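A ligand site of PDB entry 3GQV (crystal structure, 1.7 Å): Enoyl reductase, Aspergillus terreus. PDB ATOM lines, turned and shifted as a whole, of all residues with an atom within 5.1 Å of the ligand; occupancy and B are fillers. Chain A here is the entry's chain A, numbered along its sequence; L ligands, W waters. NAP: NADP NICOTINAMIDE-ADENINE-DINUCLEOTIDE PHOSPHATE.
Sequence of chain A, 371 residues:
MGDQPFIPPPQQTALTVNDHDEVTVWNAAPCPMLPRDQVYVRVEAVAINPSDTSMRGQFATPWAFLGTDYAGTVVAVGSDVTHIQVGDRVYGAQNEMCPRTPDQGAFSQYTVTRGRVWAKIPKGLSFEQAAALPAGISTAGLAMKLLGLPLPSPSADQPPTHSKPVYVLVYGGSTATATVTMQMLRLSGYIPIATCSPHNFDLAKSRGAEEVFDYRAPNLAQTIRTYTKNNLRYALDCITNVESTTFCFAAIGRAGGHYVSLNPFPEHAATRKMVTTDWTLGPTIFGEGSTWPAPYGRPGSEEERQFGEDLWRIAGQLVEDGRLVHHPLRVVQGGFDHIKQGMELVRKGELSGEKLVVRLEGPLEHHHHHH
The side-chain hydroxyl (OG) of Ser 174 lies within hydrogen-bond range of an oxygen (O2X) of the ligand (2.7 Å).
The backbone carbonyl oxygen (O) of Leu 351 sits at hydrogen-bond distance from an oxygen (O3B) of the ligand (3.2 Å).
O2D of the ligand sits at hydrogen-bond distance from OG of Ser 51, 3.4 Å away.
The side-chain hydroxyl (OG) of Ser 352 is in hydrogen-bond range of an oxygen (O3X) of the ligand.
The backbone carbonyl oxygen (O) of Leu 262 is in hydrogen-bond range of a nitrogen (N7N) of the ligand, at 2.7 Å.
The side-chain amide nitrogen of Asn 263 lies within hydrogen-bond range of an oxygen (O3D) of the ligand.
The backbone NH of Ala 176 lies within hydrogen-bond range of an oxygen (O1A) of the ligand.
O of Thr 280 is in hydrogen-bond range of N7N of the ligand (3.3 Å).
OG of Ser 197 is in hydrogen-bond range of O1X of the ligand, at 2.6 Å.
The side-chain hydroxyl (OG1) of Thr 177 lies within hydrogen-bond range of an oxygen (O1N) of the ligand (2.6 Å).
O2X of the ligand is in hydrogen-bond range of N of Ser 197, 3.0 Å away.
An oxygen (O1N) of the ligand is in hydrogen-bond range of the backbone NH of Thr 177, 2.9 Å away.
N6A of the ligand sits close to ND2 of Asn 241, at 3.4 Å.
An oxygen (O2X) of the ligand sits at hydrogen-bond distance from the side-chain amide nitrogen (ND2) of Asn 200.
NE2 of His 199 lies close to ND2 of Asn 200 (3.5 Å).
The backbone carbonyl oxygen of Leu 262 sits at hydrogen-bond distance from the side-chain hydroxyl of Thr 280, 3.3 Å away.
The guanidinium group (NH2) of Arg 216 sits at hydrogen-bond distance from the side-chain hydroxyl (OH) of Tyr 215 (3.1 Å).
The side-chain hydroxyl (OG) of Ser 352 lies within hydrogen-bond range of the side-chain amide nitrogen (ND2) of Asn 200, 2.9 Å away.
The side-chain hydroxyl of Ser 352 sits at hydrogen-bond distance from a ring nitrogen (NE2) of His 199 (3.0 Å).
O of Ser 174 lies close to NE2 of His 327 (3.4 Å).
The side-chain hydroxyl (OG) of Ser 174 lies within hydrogen-bond range of the side-chain amide nitrogen (ND2) of Asn 200.
The backbone NH (N) of Ala 178 is in hydrogen-bond range of the side-chain hydroxyl (OG1) of Thr 175.
Residues that only touch the ligand: Pro 50 (3.3 Å), Thr 139 (3.3 Å), Thr 175 (3.3 Å), Cys 196 (3.6 Å), His 199 (3.9 Å), Tyr 215 (3.4 Å), Cys 238 (3.2 Å), Ile 239 (3.5 Å), Gly 282 (3.3 Å) and Gly 353 (3.8 Å).
Hydrophobic or aromatic side chains that line the ligand: Pro 50, Ala 176, Tyr 215, Ile 239 and Leu 262.
22 residues have an atom within 4 Å of the ligand: Pro 50, Ser 51, Thr 139, Ser 174, Thr 175, Ala 176, Thr 177, Cys 196, Ser 197, His 199, Asn 200, Tyr 215, Cys 238, Ile 239, Asn 241, Leu 262, Asn 263, Thr 280, Gly 282, Leu 351, Ser 352 and Gly 353.
Water W9 lies within hydrogen-bond range of O1X of the ligand (2.6 Å), OH of Tyr 215 (2.7 Å) and NH2 of Arg 216 (3.5 Å).
Water W7 lies within hydrogen-bond range of the side-chain hydroxyl (OH) of Tyr 171 and a nitrogen (N1A) of the ligand.
Water W14 lies within hydrogen-bond range of a nitrogen (N7N) of the ligand (2.7 Å), the backbone carbonyl oxygen of Thr 280 (2.8 Å) and the backbone carbonyl oxygen of Leu 262 (3.4 Å).
Water W15 bridges OG1 of Thr 139 (2.7 Å) and O7N of the ligand (2.8 Å).
Water W12 bridges the backbone NH (N) of Gly 282 and a nitrogen (N7N) of the ligand.
Water W5 bridges N6A of the ligand (3.1 Å) and ND2 of Asn 241 (3.2 Å).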
ATOM      1  N   ASN A  49     -22.148   2.037  18.457  1.00  0.00           N
ATOM      2  CA  ASN A  49     -22.647   1.864  17.084  1.00  0.00           C
ATOM      3  C   ASN A  49     -22.897   3.209  16.402  1.00  0.00           C
ATOM      4  O   ASN A  49     -23.354   4.159  17.043  1.00  0.00           O
ATOM      5  CB  ASN A  49     -23.947   1.059  17.120  1.00  0.00           C
ATOM      6  CG  ASN A  49     -23.707  -0.412  17.461  1.00  0.00           C
ATOM      7  OD1 ASN A  49     -23.354  -1.213  16.596  1.00  0.00           O
ATOM      8  ND2 ASN A  49     -23.896  -0.778  18.738  1.00  0.00           N
ATOM      9  N   PRO A  50     -22.612   3.301  15.089  1.00  0.00           N
ATOM     10  CA  PRO A  50     -22.885   4.560  14.387  1.00  0.00           C
ATOM     11  C   PRO A  50     -24.297   5.085  14.607  1.00  0.00           C
ATOM     12  O   PRO A  50     -24.484   6.310  14.687  1.00  0.00           O
ATOM     13  CB  PRO A  50     -22.682   4.200  12.913  1.00  0.00           C
ATOM     14  CG  PRO A  50     -21.641   3.143  12.955  1.00  0.00           C
ATOM     15  CD  PRO A  50     -21.976   2.321  14.199  1.00  0.00           C
ATOM     16  N   SER A  51     -25.274   4.189  14.737  1.00  0.00           N
ATOM     17  CA  SER A  51     -26.645   4.617  14.941  1.00  0.00           C
ATOM     18  C   SER A  51     -26.863   5.322  16.295  1.00  0.00           C
ATOM     19  O   SER A  51     -27.805   6.093  16.450  1.00  0.00           O
ATOM     20  CB  SER A  51     -27.617   3.450  14.712  1.00  0.00           C
ATOM     21  OG  SER A  51     -27.423   2.949  13.393  1.00  0.00           O
ATOM     22  N   THR A 139     -28.735  -7.120  13.079  1.00  0.00           N
ATOM     23  CA  THR A 139     -28.715  -6.529  11.729  1.00  0.00           C
ATOM     24  C   THR A 139     -28.455  -7.595  10.647  1.00  0.00           C
ATOM     25  O   THR A 139     -29.135  -7.609   9.602  1.00  0.00           O
ATOM     26  CB  THR A 139     -27.700  -5.337  11.669  1.00  0.00           C
ATOM     27  OG1 THR A 139     -27.959  -4.430  12.736  1.00  0.00           O
ATOM     28  CG2 THR A 139     -27.834  -4.590  10.352  1.00  0.00           C
ATOM     29  N   TYR A 171     -21.080  -4.787   0.143  1.00  0.00           N
ATOM     30  CA  TYR A 171     -20.368  -3.525  -0.072  1.00  0.00           C
ATOM     31  C   TYR A 171     -20.073  -2.973   1.319  1.00  0.00           C
ATOM     32  O   TYR A 171     -21.003  -2.655   2.080  1.00  0.00           O
ATOM     33  CB  TYR A 171     -21.211  -2.558  -0.886  1.00  0.00           C
ATOM     34  CG  TYR A 171     -20.416  -1.356  -1.357  1.00  0.00           C
ATOM     35  CD1 TYR A 171     -19.842  -1.332  -2.646  1.00  0.00           C
ATOM     36  CD2 TYR A 171     -20.242  -0.232  -0.530  1.00  0.00           C
ATOM     37  CE1 TYR A 171     -19.089  -0.218  -3.105  1.00  0.00           C
ATOM     38  CE2 TYR A 171     -19.477   0.891  -0.961  1.00  0.00           C
ATOM     39  CZ  TYR A 171     -18.920   0.888  -2.255  1.00  0.00           C
ATOM     40  OH  TYR A 171     -18.218   1.957  -2.694  1.00  0.00           O
ATOM     41  N   SER A 174     -15.612  -4.622   5.643  1.00  0.00           N
ATOM     42  CA  SER A 174     -14.918  -4.478   6.927  1.00  0.00           C
ATOM     43  C   SER A 174     -15.808  -3.824   8.016  1.00  0.00           C
ATOM     44  O   SER A 174     -15.347  -3.589   9.125  1.00  0.00           O
ATOM     45  CB  SER A 174     -13.635  -3.649   6.768  1.00  0.00           C
ATOM     46  OG  SER A 174     -13.965  -2.282   6.599  1.00  0.00           O
ATOM     47  N   THR A 175     -17.046  -3.490   7.658  1.00  0.00           N
ATOM     48  CA  THR A 175     -17.992  -2.990   8.667  1.00  0.00           C
ATOM     49  C   THR A 175     -18.233  -4.034   9.750  1.00  0.00           C
ATOM     50  O   THR A 175     -18.207  -5.238   9.473  1.00  0.00           O
ATOM     51  CB  THR A 175     -19.346  -2.530   8.058  1.00  0.00           C
ATOM     52  OG1 THR A 175     -20.009  -3.614   7.372  1.00  0.00           O
ATOM     53  CG2 THR A 175     -19.109  -1.384   7.068  1.00  0.00           C
ATOM     54  N   ALA A 176     -18.526  -3.551  10.960  1.00  0.00           N
ATOM     55  CA  ALA A 176     -18.978  -4.460  12.034  1.00  0.00           C
ATOM     56  C   ALA A 176     -20.160  -5.372  11.582  1.00  0.00           C
ATOM     57  O   ALA A 176     -20.144  -6.587  11.833  1.00  0.00           O
ATOM     58  CB  ALA A 176     -19.355  -3.655  13.285  1.00  0.00           C
ATOM     59  N   THR A 177     -21.146  -4.794  10.911  1.00  0.00           N
ATOM     60  CA  THR A 177     -22.276  -5.594  10.393  1.00  0.00           C
ATOM     61  C   THR A 177     -21.779  -6.653   9.394  1.00  0.00           C
ATOM     62  O   THR A 177     -22.160  -7.827   9.504  1.00  0.00           O
ATOM     63  CB  THR A 177     -23.353  -4.711   9.724  1.00  0.00           C
ATOM     64  OG1 THR A 177     -23.769  -3.700  10.647  1.00  0.00           O
ATOM     65  CG2 THR A 177     -24.590  -5.552   9.292  1.00  0.00           C
ATOM     66  N   ALA A 178     -20.921  -6.266   8.435  1.00  0.00           N
ATOM     67  CA  ALA A 178     -20.507  -7.225   7.386  1.00  0.00           C
ATOM     68  C   ALA A 178     -19.752  -8.426   7.937  1.00  0.00           C
ATOM     69  O   ALA A 178     -19.912  -9.539   7.451  1.00  0.00           O
ATOM     70  CB  ALA A 178     -19.638  -6.552   6.308  1.00  0.00           C
ATOM     71  N   CYS A 196     -13.838  -3.376   0.350  1.00  0.00           N
ATOM     72  CA  CYS A 196     -13.405  -2.585   1.513  1.00  0.00           C
ATOM     73  C   CYS A 196     -12.016  -2.033   1.217  1.00  0.00           C
ATOM     74  O   CYS A 196     -11.571  -2.107   0.063  1.00  0.00           O
ATOM     75  CB  CYS A 196     -13.413  -3.455   2.786  1.00  0.00           C
ATOM     76  SG  CYS A 196     -12.236  -4.843   2.813  1.00  0.00           S
ATOM     77  N   SER A 197     -11.352  -1.424   2.208  1.00  0.00           N
ATOM     78  CA  SER A 197      -9.999  -0.930   1.952  1.00  0.00           C
ATOM     79  C   SER A 197      -8.983  -2.049   2.073  1.00  0.00           C
ATOM     80  O   SER A 197      -9.178  -2.999   2.839  1.00  0.00           O
ATOM     81  CB  SER A 197      -9.631   0.242   2.885  1.00  0.00           C
ATOM     82  OG  SER A 197     -10.418   1.386   2.604  1.00  0.00           O
ATOM     83  N   HIS A 199      -6.223  -2.540   3.620  1.00  0.00           N
ATOM     84  CA  HIS A 199      -5.695  -2.975   4.915  1.00  0.00           C
ATOM     85  C   HIS A 199      -6.632  -3.918   5.672  1.00  0.00           C
ATOM     86  O   HIS A 199      -6.180  -4.667   6.539  1.00  0.00           O
ATOM     87  CB  HIS A 199      -5.227  -1.796   5.775  1.00  0.00           C
ATOM     88  CG  HIS A 199      -6.341  -1.029   6.415  1.00  0.00           C
ATOM     89  ND1 HIS A 199      -6.784  -1.284   7.700  1.00  0.00           N
ATOM     90  CD2 HIS A 199      -7.100  -0.005   5.950  1.00  0.00           C
ATOM     91  CE1 HIS A 199      -7.765  -0.454   7.995  1.00  0.00           C
ATOM     92  NE2 HIS A 199      -7.982   0.327   6.957  1.00  0.00           N
ATOM     93  N   ASN A 200      -7.917  -3.915   5.309  1.00  0.00           N
ATOM     94  CA  ASN A 200      -8.886  -4.832   5.885  1.00  0.00           C
ATOM     95  C   ASN A 200      -9.181  -6.100   5.034  1.00  0.00           C
ATOM     96  O   ASN A 200     -10.093  -6.861   5.346  1.00  0.00           O
ATOM     97  CB  ASN A 200     -10.193  -4.072   6.172  1.00  0.00           C
ATOM     98  CG  ASN A 200     -10.058  -3.075   7.339  1.00  0.00           C
ATOM     99  OD1 ASN A 200      -9.462  -3.398   8.373  1.00  0.00           O
ATOM    100  ND2 ASN A 200     -10.623  -1.898   7.182  1.00  0.00           N
ATOM    101  N   TYR A 215     -12.869  -0.930  -3.033  1.00  0.00           N
ATOM    102  CA  TYR A 215     -14.030  -0.265  -3.662  1.00  0.00           C
ATOM    103  C   TYR A 215     -13.653   0.923  -4.571  1.00  0.00           C
ATOM    104  O   TYR A 215     -14.462   1.337  -5.398  1.00  0.00           O
ATOM    105  CB  TYR A 215     -15.086   0.182  -2.626  1.00  0.00           C
ATOM    106  CG  TYR A 215     -14.618   1.294  -1.720  1.00  0.00           C
ATOM    107  CD1 TYR A 215     -14.847   2.630  -2.049  1.00  0.00           C
ATOM    108  CD2 TYR A 215     -13.946   1.010  -0.526  1.00  0.00           C
ATOM    109  CE1 TYR A 215     -14.414   3.659  -1.212  1.00  0.00           C
ATOM    110  CE2 TYR A 215     -13.506   2.047   0.320  1.00  0.00           C
ATOM    111  CZ  TYR A 215     -13.739   3.353  -0.036  1.00  0.00           C
ATOM    112  OH  TYR A 215     -13.316   4.375   0.793  1.00  0.00           O
ATOM    113  N   ARG A 216     -12.432   1.447  -4.401  1.00  0.00           N
ATOM    114  CA  ARG A 216     -11.953   2.589  -5.196  1.00  0.00           C
ATOM    115  C   ARG A 216     -11.468   2.181  -6.597  1.00  0.00           C
ATOM    116  O   ARG A 216     -11.194   3.054  -7.435  1.00  0.00           O
ATOM    117  CB  ARG A 216     -10.805   3.272  -4.477  1.00  0.00           C
ATOM    118  CG  ARG A 216     -11.131   3.791  -3.064  1.00  0.00           C
ATOM    119  CD  ARG A 216      -9.810   4.043  -2.345  1.00  0.00           C
ATOM    120  NE  ARG A 216      -9.980   4.511  -0.975  1.00  0.00           N
ATOM    121  CZ  ARG A 216     -10.154   3.710   0.088  1.00  0.00           C
ATOM    122  NH1 ARG A 216     -10.218   2.375  -0.065  1.00  0.00           N
ATOM    123  NH2 ARG A 216     -10.249   4.243   1.303  1.00  0.00           N
ATOM    124  N   CYS A 238     -23.657  -2.095   3.152  1.00  0.00           N
ATOM    125  CA  CYS A 238     -23.355  -1.735   4.551  1.00  0.00           C
ATOM    126  C   CYS A 238     -22.882  -0.298   4.720  1.00  0.00           C
ATOM    127  O   CYS A 238     -22.577   0.106   5.841  1.00  0.00           O
ATOM    128  CB  CYS A 238     -22.308  -2.683   5.128  1.00  0.00           C
ATOM    129  SG  CYS A 238     -22.840  -4.435   5.115  1.00  0.00           S
ATOM    130  N   ILE A 239     -22.802   0.449   3.622  1.00  0.00           N
ATOM    131  CA  ILE A 239     -22.352   1.854   3.655  1.00  0.00           C
ATOM    132  C   ILE A 239     -23.493   2.864   3.436  1.00  0.00           C
ATOM    133  O   ILE A 239     -23.607   3.886   4.173  1.00  0.00           O
ATOM    134  CB  ILE A 239     -21.173   2.069   2.625  1.00  0.00           C
ATOM    135  CG1 ILE A 239     -20.005   1.107   2.927  1.00  0.00           C
ATOM    136  CG2 ILE A 239     -20.758   3.550   2.544  1.00  0.00           C
ATOM    137  CD1 ILE A 239     -19.442   1.165   4.395  1.00  0.00           C
ATOM    138  N   ASN A 241     -24.612   5.185   0.720  1.00  0.00           N
ATOM    139  CA  ASN A 241     -24.485   6.538   0.228  1.00  0.00           C
ATOM    140  C   ASN A 241     -24.659   6.499  -1.284  1.00  0.00           C
ATOM    141  O   ASN A 241     -24.924   5.441  -1.865  1.00  0.00           O
ATOM    142  CB  ASN A 241     -23.177   7.214   0.698  1.00  0.00           C
ATOM    143  CG  ASN A 241     -21.927   6.512   0.159  1.00  0.00           C
ATOM    144  OD1 ASN A 241     -21.972   5.857  -0.877  1.00  0.00           O
ATOM    145  ND2 ASN A 241     -20.809   6.668   0.849  1.00  0.00           N
ATOM    146  N   LEU A 262     -28.456  -0.878   4.776  1.00  0.00           N
ATOM    147  CA  LEU A 262     -28.627  -0.847   6.257  1.00  0.00           C
ATOM    148  C   LEU A 262     -29.267   0.461   6.794  1.00  0.00           C
ATOM    149  O   LEU A 262     -29.601   0.551   7.975  1.00  0.00           O
ATOM    150  CB  LEU A 262     -27.292  -1.098   6.950  1.00  0.00           C
ATOM    151  CG  LEU A 262     -26.581  -2.412   6.618  1.00  0.00           C
ATOM    152  CD1 LEU A 262     -25.301  -2.552   7.449  1.00  0.00           C
ATOM    153  CD2 LEU A 262     -27.560  -3.613   6.827  1.00  0.00           C
ATOM    154  N   ASN A 263     -29.355   1.471   5.933  1.00  0.00           N
ATOM    155  CA  ASN A 263     -29.964   2.780   6.214  1.00  0.00           C
ATOM    156  C   ASN A 263     -30.975   3.101   5.094  1.00  0.00           C
ATOM    157  O   ASN A 263     -30.861   2.570   3.989  1.00  0.00           O
ATOM    158  CB  ASN A 263     -28.883   3.884   6.245  1.00  0.00           C
ATOM    159  CG  ASN A 263     -27.947   3.828   7.470  1.00  0.00           C
ATOM    160  OD1 ASN A 263     -28.385   3.591   8.581  1.00  0.00           O
ATOM    161  ND2 ASN A 263     -26.641   4.123   7.257  1.00  0.00           N
ATOM    162  N   THR A 280     -33.020  -2.165   6.230  1.00  0.00           N
ATOM    163  CA  THR A 280     -33.251  -2.700   7.568  1.00  0.00           C
ATOM    164  C   THR A 280     -33.671  -1.601   8.524  1.00  0.00           C
ATOM    165  O   THR A 280     -33.024  -0.541   8.597  1.00  0.00           O
ATOM    166  CB  THR A 280     -31.990  -3.398   8.158  1.00  0.00           C
ATOM    167  OG1 THR A 280     -30.906  -2.463   8.205  1.00  0.00           O
ATOM    168  CG2 THR A 280     -31.581  -4.640   7.338  1.00  0.00           C
ATOM    169  N   LEU A 281     -34.737  -1.875   9.253  1.00  0.00           N
ATOM    170  CA  LEU A 281     -35.227  -0.995  10.318  1.00  0.00           C
ATOM    171  C   LEU A 281     -34.946  -1.695  11.634  1.00  0.00           C
ATOM    172  O   LEU A 281     -35.613  -2.668  11.990  1.00  0.00           O
ATOM    173  CB  LEU A 281     -36.739  -0.766  10.142  1.00  0.00           C
ATOM    174  CG  LEU A 281     -37.452   0.173  11.145  1.00  0.00           C
ATOM    175  CD1 LEU A 281     -36.812   1.570  11.238  1.00  0.00           C
ATOM    176  CD2 LEU A 281     -38.933   0.298  10.803  1.00  0.00           C
ATOM    177  N   GLY A 282     -33.947  -1.180  12.345  1.00  0.00           N
ATOM    178  CA  GLY A 282     -33.366  -1.845  13.503  1.00  0.00           C
ATOM    179  C   GLY A 282     -34.361  -2.245  14.600  1.00  0.00           C
ATOM    180  O   GLY A 282     -34.300  -3.397  15.093  1.00  0.00           O
ATOM    181  N   HIS A 327     -16.576  -8.914  15.965  1.00  0.00           N
ATOM    182  CA  HIS A 327     -15.746  -8.010  15.163  1.00  0.00           C
ATOM    183  C   HIS A 327     -14.500  -7.719  16.018  1.00  0.00           C
ATOM    184  O   HIS A 327     -14.585  -7.796  17.257  1.00  0.00           O
ATOM    185  CB  HIS A 327     -16.539  -6.726  14.931  1.00  0.00           C
ATOM    186  CG  HIS A 327     -16.030  -5.860  13.815  1.00  0.00           C
ATOM    187  ND1 HIS A 327     -15.943  -6.295  12.512  1.00  0.00           N
ATOM    188  CD2 HIS A 327     -15.701  -4.559  13.800  1.00  0.00           C
ATOM    189  CE1 HIS A 327     -15.530  -5.302  11.748  1.00  0.00           C
ATOM    190  NE2 HIS A 327     -15.361  -4.235  12.500  1.00  0.00           N
ATOM    191  N   LEU A 351     -12.824   4.935  13.134  1.00  0.00           N
ATOM    192  CA  LEU A 351     -12.540   3.528  13.363  1.00  0.00           C
ATOM    193  C   LEU A 351     -12.595   2.759  12.046  1.00  0.00           C
ATOM    194  O   LEU A 351     -13.543   2.923  11.247  1.00  0.00           O
ATOM    195  CB  LEU A 351     -13.527   2.911  14.358  1.00  0.00           C
ATOM    196  CG  LEU A 351     -13.447   3.211  15.857  1.00  0.00           C
ATOM    197  CD1 LEU A 351     -14.579   2.497  16.564  1.00  0.00           C
ATOM    198  CD2 LEU A 351     -12.117   2.798  16.485  1.00  0.00           C
ATOM    199  N   SER A 352     -11.585   1.928  11.828  1.00  0.00           N
ATOM    200  CA  SER A 352     -11.541   1.020  10.684  1.00  0.00           C
ATOM    201  C   SER A 352     -11.238  -0.411  11.115  1.00  0.00           C
ATOM    202  O   SER A 352     -10.205  -0.685  11.723  1.00  0.00           O
ATOM    203  CB  SER A 352     -10.517   1.524   9.655  1.00  0.00           C
ATOM    204  OG  SER A 352     -10.509   0.664   8.531  1.00  0.00           O
ATOM    205  N   GLY A 353     -12.155  -1.319  10.805  1.00  0.00           N
ATOM    206  CA  GLY A 353     -11.988  -2.748  11.090  1.00  0.00           C
ATOM    207  C   GLY A 353     -11.991  -3.099  12.567  1.00  0.00           C
ATOM    208  O   GLY A 353     -11.402  -4.111  12.968  1.00  0.00           O
ATOM    209  N   GLU A 354     -12.609  -2.249  13.386  1.00  0.00           N
ATOM    210  CA  GLU A 354     -12.706  -2.497  14.834  1.00  0.00           C
ATOM    211  C   GLU A 354     -13.997  -1.961  15.393  1.00  0.00           C
ATOM    212  O   GLU A 354     -14.595  -1.036  14.829  1.00  0.00           O
ATOM    213  CB  GLU A 354     -11.581  -1.806  15.606  1.00  0.00           C
ATOM    214  CG  GLU A 354     -10.208  -1.955  15.063  1.00  0.00           C
ATOM    215  CD  GLU A 354      -9.191  -1.266  15.957  1.00  0.00           C
ATOM    216  OE1 GLU A 354      -9.108  -0.019  15.945  1.00  0.00           O
ATOM    217  OE2 GLU A 354      -8.491  -1.999  16.664  1.00  0.00           O
ATOM    218  N   LYS A 355     -14.387  -2.526  16.529  1.00  0.00           N
ATOM    219  CA  LYS A 355     -15.569  -2.135  17.281  1.00  0.00           C
ATOM    220  C   LYS A 355     -15.096  -1.455  18.570  1.00  0.00           C
ATOM    221  O   LYS A 355     -14.304  -2.043  19.294  1.00  0.00           O
ATOM    222  CB  LYS A 355     -16.358  -3.398  17.646  1.00  0.00           C
ATOM    223  CG  LYS A 355     -17.769  -3.151  18.225  1.00  0.00           C
ATOM    224  CD  LYS A 355     -18.787  -3.100  17.101  1.00  0.00           C
ATOM    225  CE  LYS A 355     -20.135  -2.575  17.586  1.00  0.00           C
ATOM    226  NZ  LYS A 355     -20.999  -2.232  16.428  1.00  0.00           N
HETATM  227  PA  NAP L   1     -18.653   0.340  10.971  1.00  0.00           P
HETATM  228  O1A NAP L   1     -17.829  -0.655  11.698  1.00  0.00           O
HETATM  229  O2A NAP L   1     -18.824   1.642  11.628  1.00  0.00           O
HETATM  230  O5B NAP L   1     -17.988   0.628   9.527  1.00  0.00           O
HETATM  231  C5B NAP L   1     -16.817   1.388   9.377  1.00  0.00           C
HETATM  232  C4B NAP L   1     -16.219   1.116   7.992  1.00  0.00           C
HETATM  233  O4B NAP L   1     -16.972   1.580   6.912  1.00  0.00           O
HETATM  234  C3B NAP L   1     -14.907   1.853   7.849  1.00  0.00           C
HETATM  235  O3B NAP L   1     -13.953   1.140   8.577  1.00  0.00           O
HETATM  236  C2B NAP L   1     -14.661   1.779   6.354  1.00  0.00           C
HETATM  237  O2B NAP L   1     -14.075   0.544   5.937  1.00  0.00           O
HETATM  238  C1B NAP L   1     -16.071   1.808   5.810  1.00  0.00           C
HETATM  239  N9A NAP L   1     -16.453   3.065   5.151  1.00  0.00           N
HETATM  240  C8A NAP L   1     -16.752   4.284   5.740  1.00  0.00           C
HETATM  241  N7A NAP L   1     -17.116   5.175   4.789  1.00  0.00           N
HETATM  242  C5A NAP L   1     -17.035   4.523   3.587  1.00  0.00           C
HETATM  243  C6A NAP L   1     -17.287   4.945   2.283  1.00  0.00           C
HETATM  244  N6A NAP L   1     -17.683   6.189   1.990  1.00  0.00           N
HETATM  245  N1A NAP L   1     -17.116   4.040   1.256  1.00  0.00           N
HETATM  246  C2A NAP L   1     -16.695   2.726   1.502  1.00  0.00           C
HETATM  247  N3A NAP L   1     -16.459   2.303   2.787  1.00  0.00           N
HETATM  248  C4A NAP L   1     -16.632   3.207   3.804  1.00  0.00           C
HETATM  249  O3  NAP L   1     -19.981  -0.368  10.456  1.00  0.00           O
HETATM  250  PN  NAP L   1     -21.404  -0.685  11.077  1.00  0.00           P
HETATM  251  O1N NAP L   1     -21.790  -2.006  10.494  1.00  0.00           O
HETATM  252  O2N NAP L   1     -21.436  -0.481  12.537  1.00  0.00           O
HETATM  253  O5D NAP L   1     -22.344   0.408  10.394  1.00  0.00           O
HETATM  254  C5D NAP L   1     -22.279   0.655   8.980  1.00  0.00           C
HETATM  255  C4D NAP L   1     -23.456   1.517   8.527  1.00  0.00           C
HETATM  256  O4D NAP L   1     -24.593   0.720   8.686  1.00  0.00           O
HETATM  257  C3D NAP L   1     -23.698   2.797   9.345  1.00  0.00           C
HETATM  258  O3D NAP L   1     -24.208   3.825   8.520  1.00  0.00           O
HETATM  259  C2D NAP L   1     -24.837   2.405  10.276  1.00  0.00           C
HETATM  260  O2D NAP L   1     -25.653   3.536  10.556  1.00  0.00           O
HETATM  261  C1D NAP L   1     -25.583   1.369   9.443  1.00  0.00           C
HETATM  262  N1N NAP L   1     -26.268   0.405  10.305  1.00  0.00           N
HETATM  263  C2N NAP L   1     -27.609   0.609  10.496  1.00  0.00           C
HETATM  264  C3N NAP L   1     -28.311  -0.251  11.320  1.00  0.00           C
HETATM  265  C7N NAP L   1     -29.812  -0.133  11.405  1.00  0.00           C
HETATM  266  O7N NAP L   1     -30.420  -0.767  12.491  1.00  0.00           O
HETATM  267  N7N NAP L   1     -30.504   0.555  10.469  1.00  0.00           N
HETATM  268  C4N NAP L   1     -27.640  -1.286  11.977  1.00  0.00           C
HETATM  269  C5N NAP L   1     -26.270  -1.477  11.792  1.00  0.00           C
HETATM  270  C6N NAP L   1     -25.584  -0.619  10.940  1.00  0.00           C
HETATM  271  P2B NAP L   1     -12.605   0.507   5.222  1.00  0.00           P
HETATM  272  O1X NAP L   1     -12.736   1.192   3.850  1.00  0.00           O
HETATM  273  O2X NAP L   1     -12.178  -0.933   5.074  1.00  0.00           O
HETATM  274  O3X NAP L   1     -11.666   1.274   6.128  1.00  0.00           O
HETATM  275  O   HOH W   1     -17.167   0.222  14.383  1.00  0.00           O
HETATM  276  O   HOH W   2     -19.727  -0.403  14.715  1.00  0.00           O
HETATM  277  O   HOH W   3      -9.236   2.313   6.005  1.00  0.00           O
HETATM  278  O   HOH W   4     -23.724  -1.047  13.935  1.00  0.00           O
HETATM  279  O   HOH W   5     -18.188   6.915  -0.950  1.00  0.00           O
HETATM  280  O   HOH W   6     -15.317  -1.526  11.408  1.00  0.00           O
HETATM  281  O   HOH W   7     -18.370   4.144  -1.150  1.00  0.00           O
HETATM  282  O   HOH W   8     -24.076   6.243  10.293  1.00  0.00           O
HETATM  283  O   HOH W   9     -13.007   3.786   3.389  1.00  0.00           O
HETATM  284  O   HOH W  10     -16.968   2.629  13.160  1.00  0.00           O
HETATM  285  O   HOH W  11     -18.635   8.505   3.631  1.00  0.00           O
HETATM  286  O   HOH W  12     -33.009   1.572  11.806  1.00  0.00           O
HETATM  287  O   HOH W  13     -11.742   3.766   6.928  1.00  0.00           O
HETATM  288  O   HOH W  14     -32.365   2.098   9.160  1.00  0.00           O
HETATM  289  O   HOH W  15     -30.468  -3.530  12.891  1.00  0.00           O
HETATM  290  O   HOH W  16     -15.121  -0.107   2.749  1.00  0.00           O
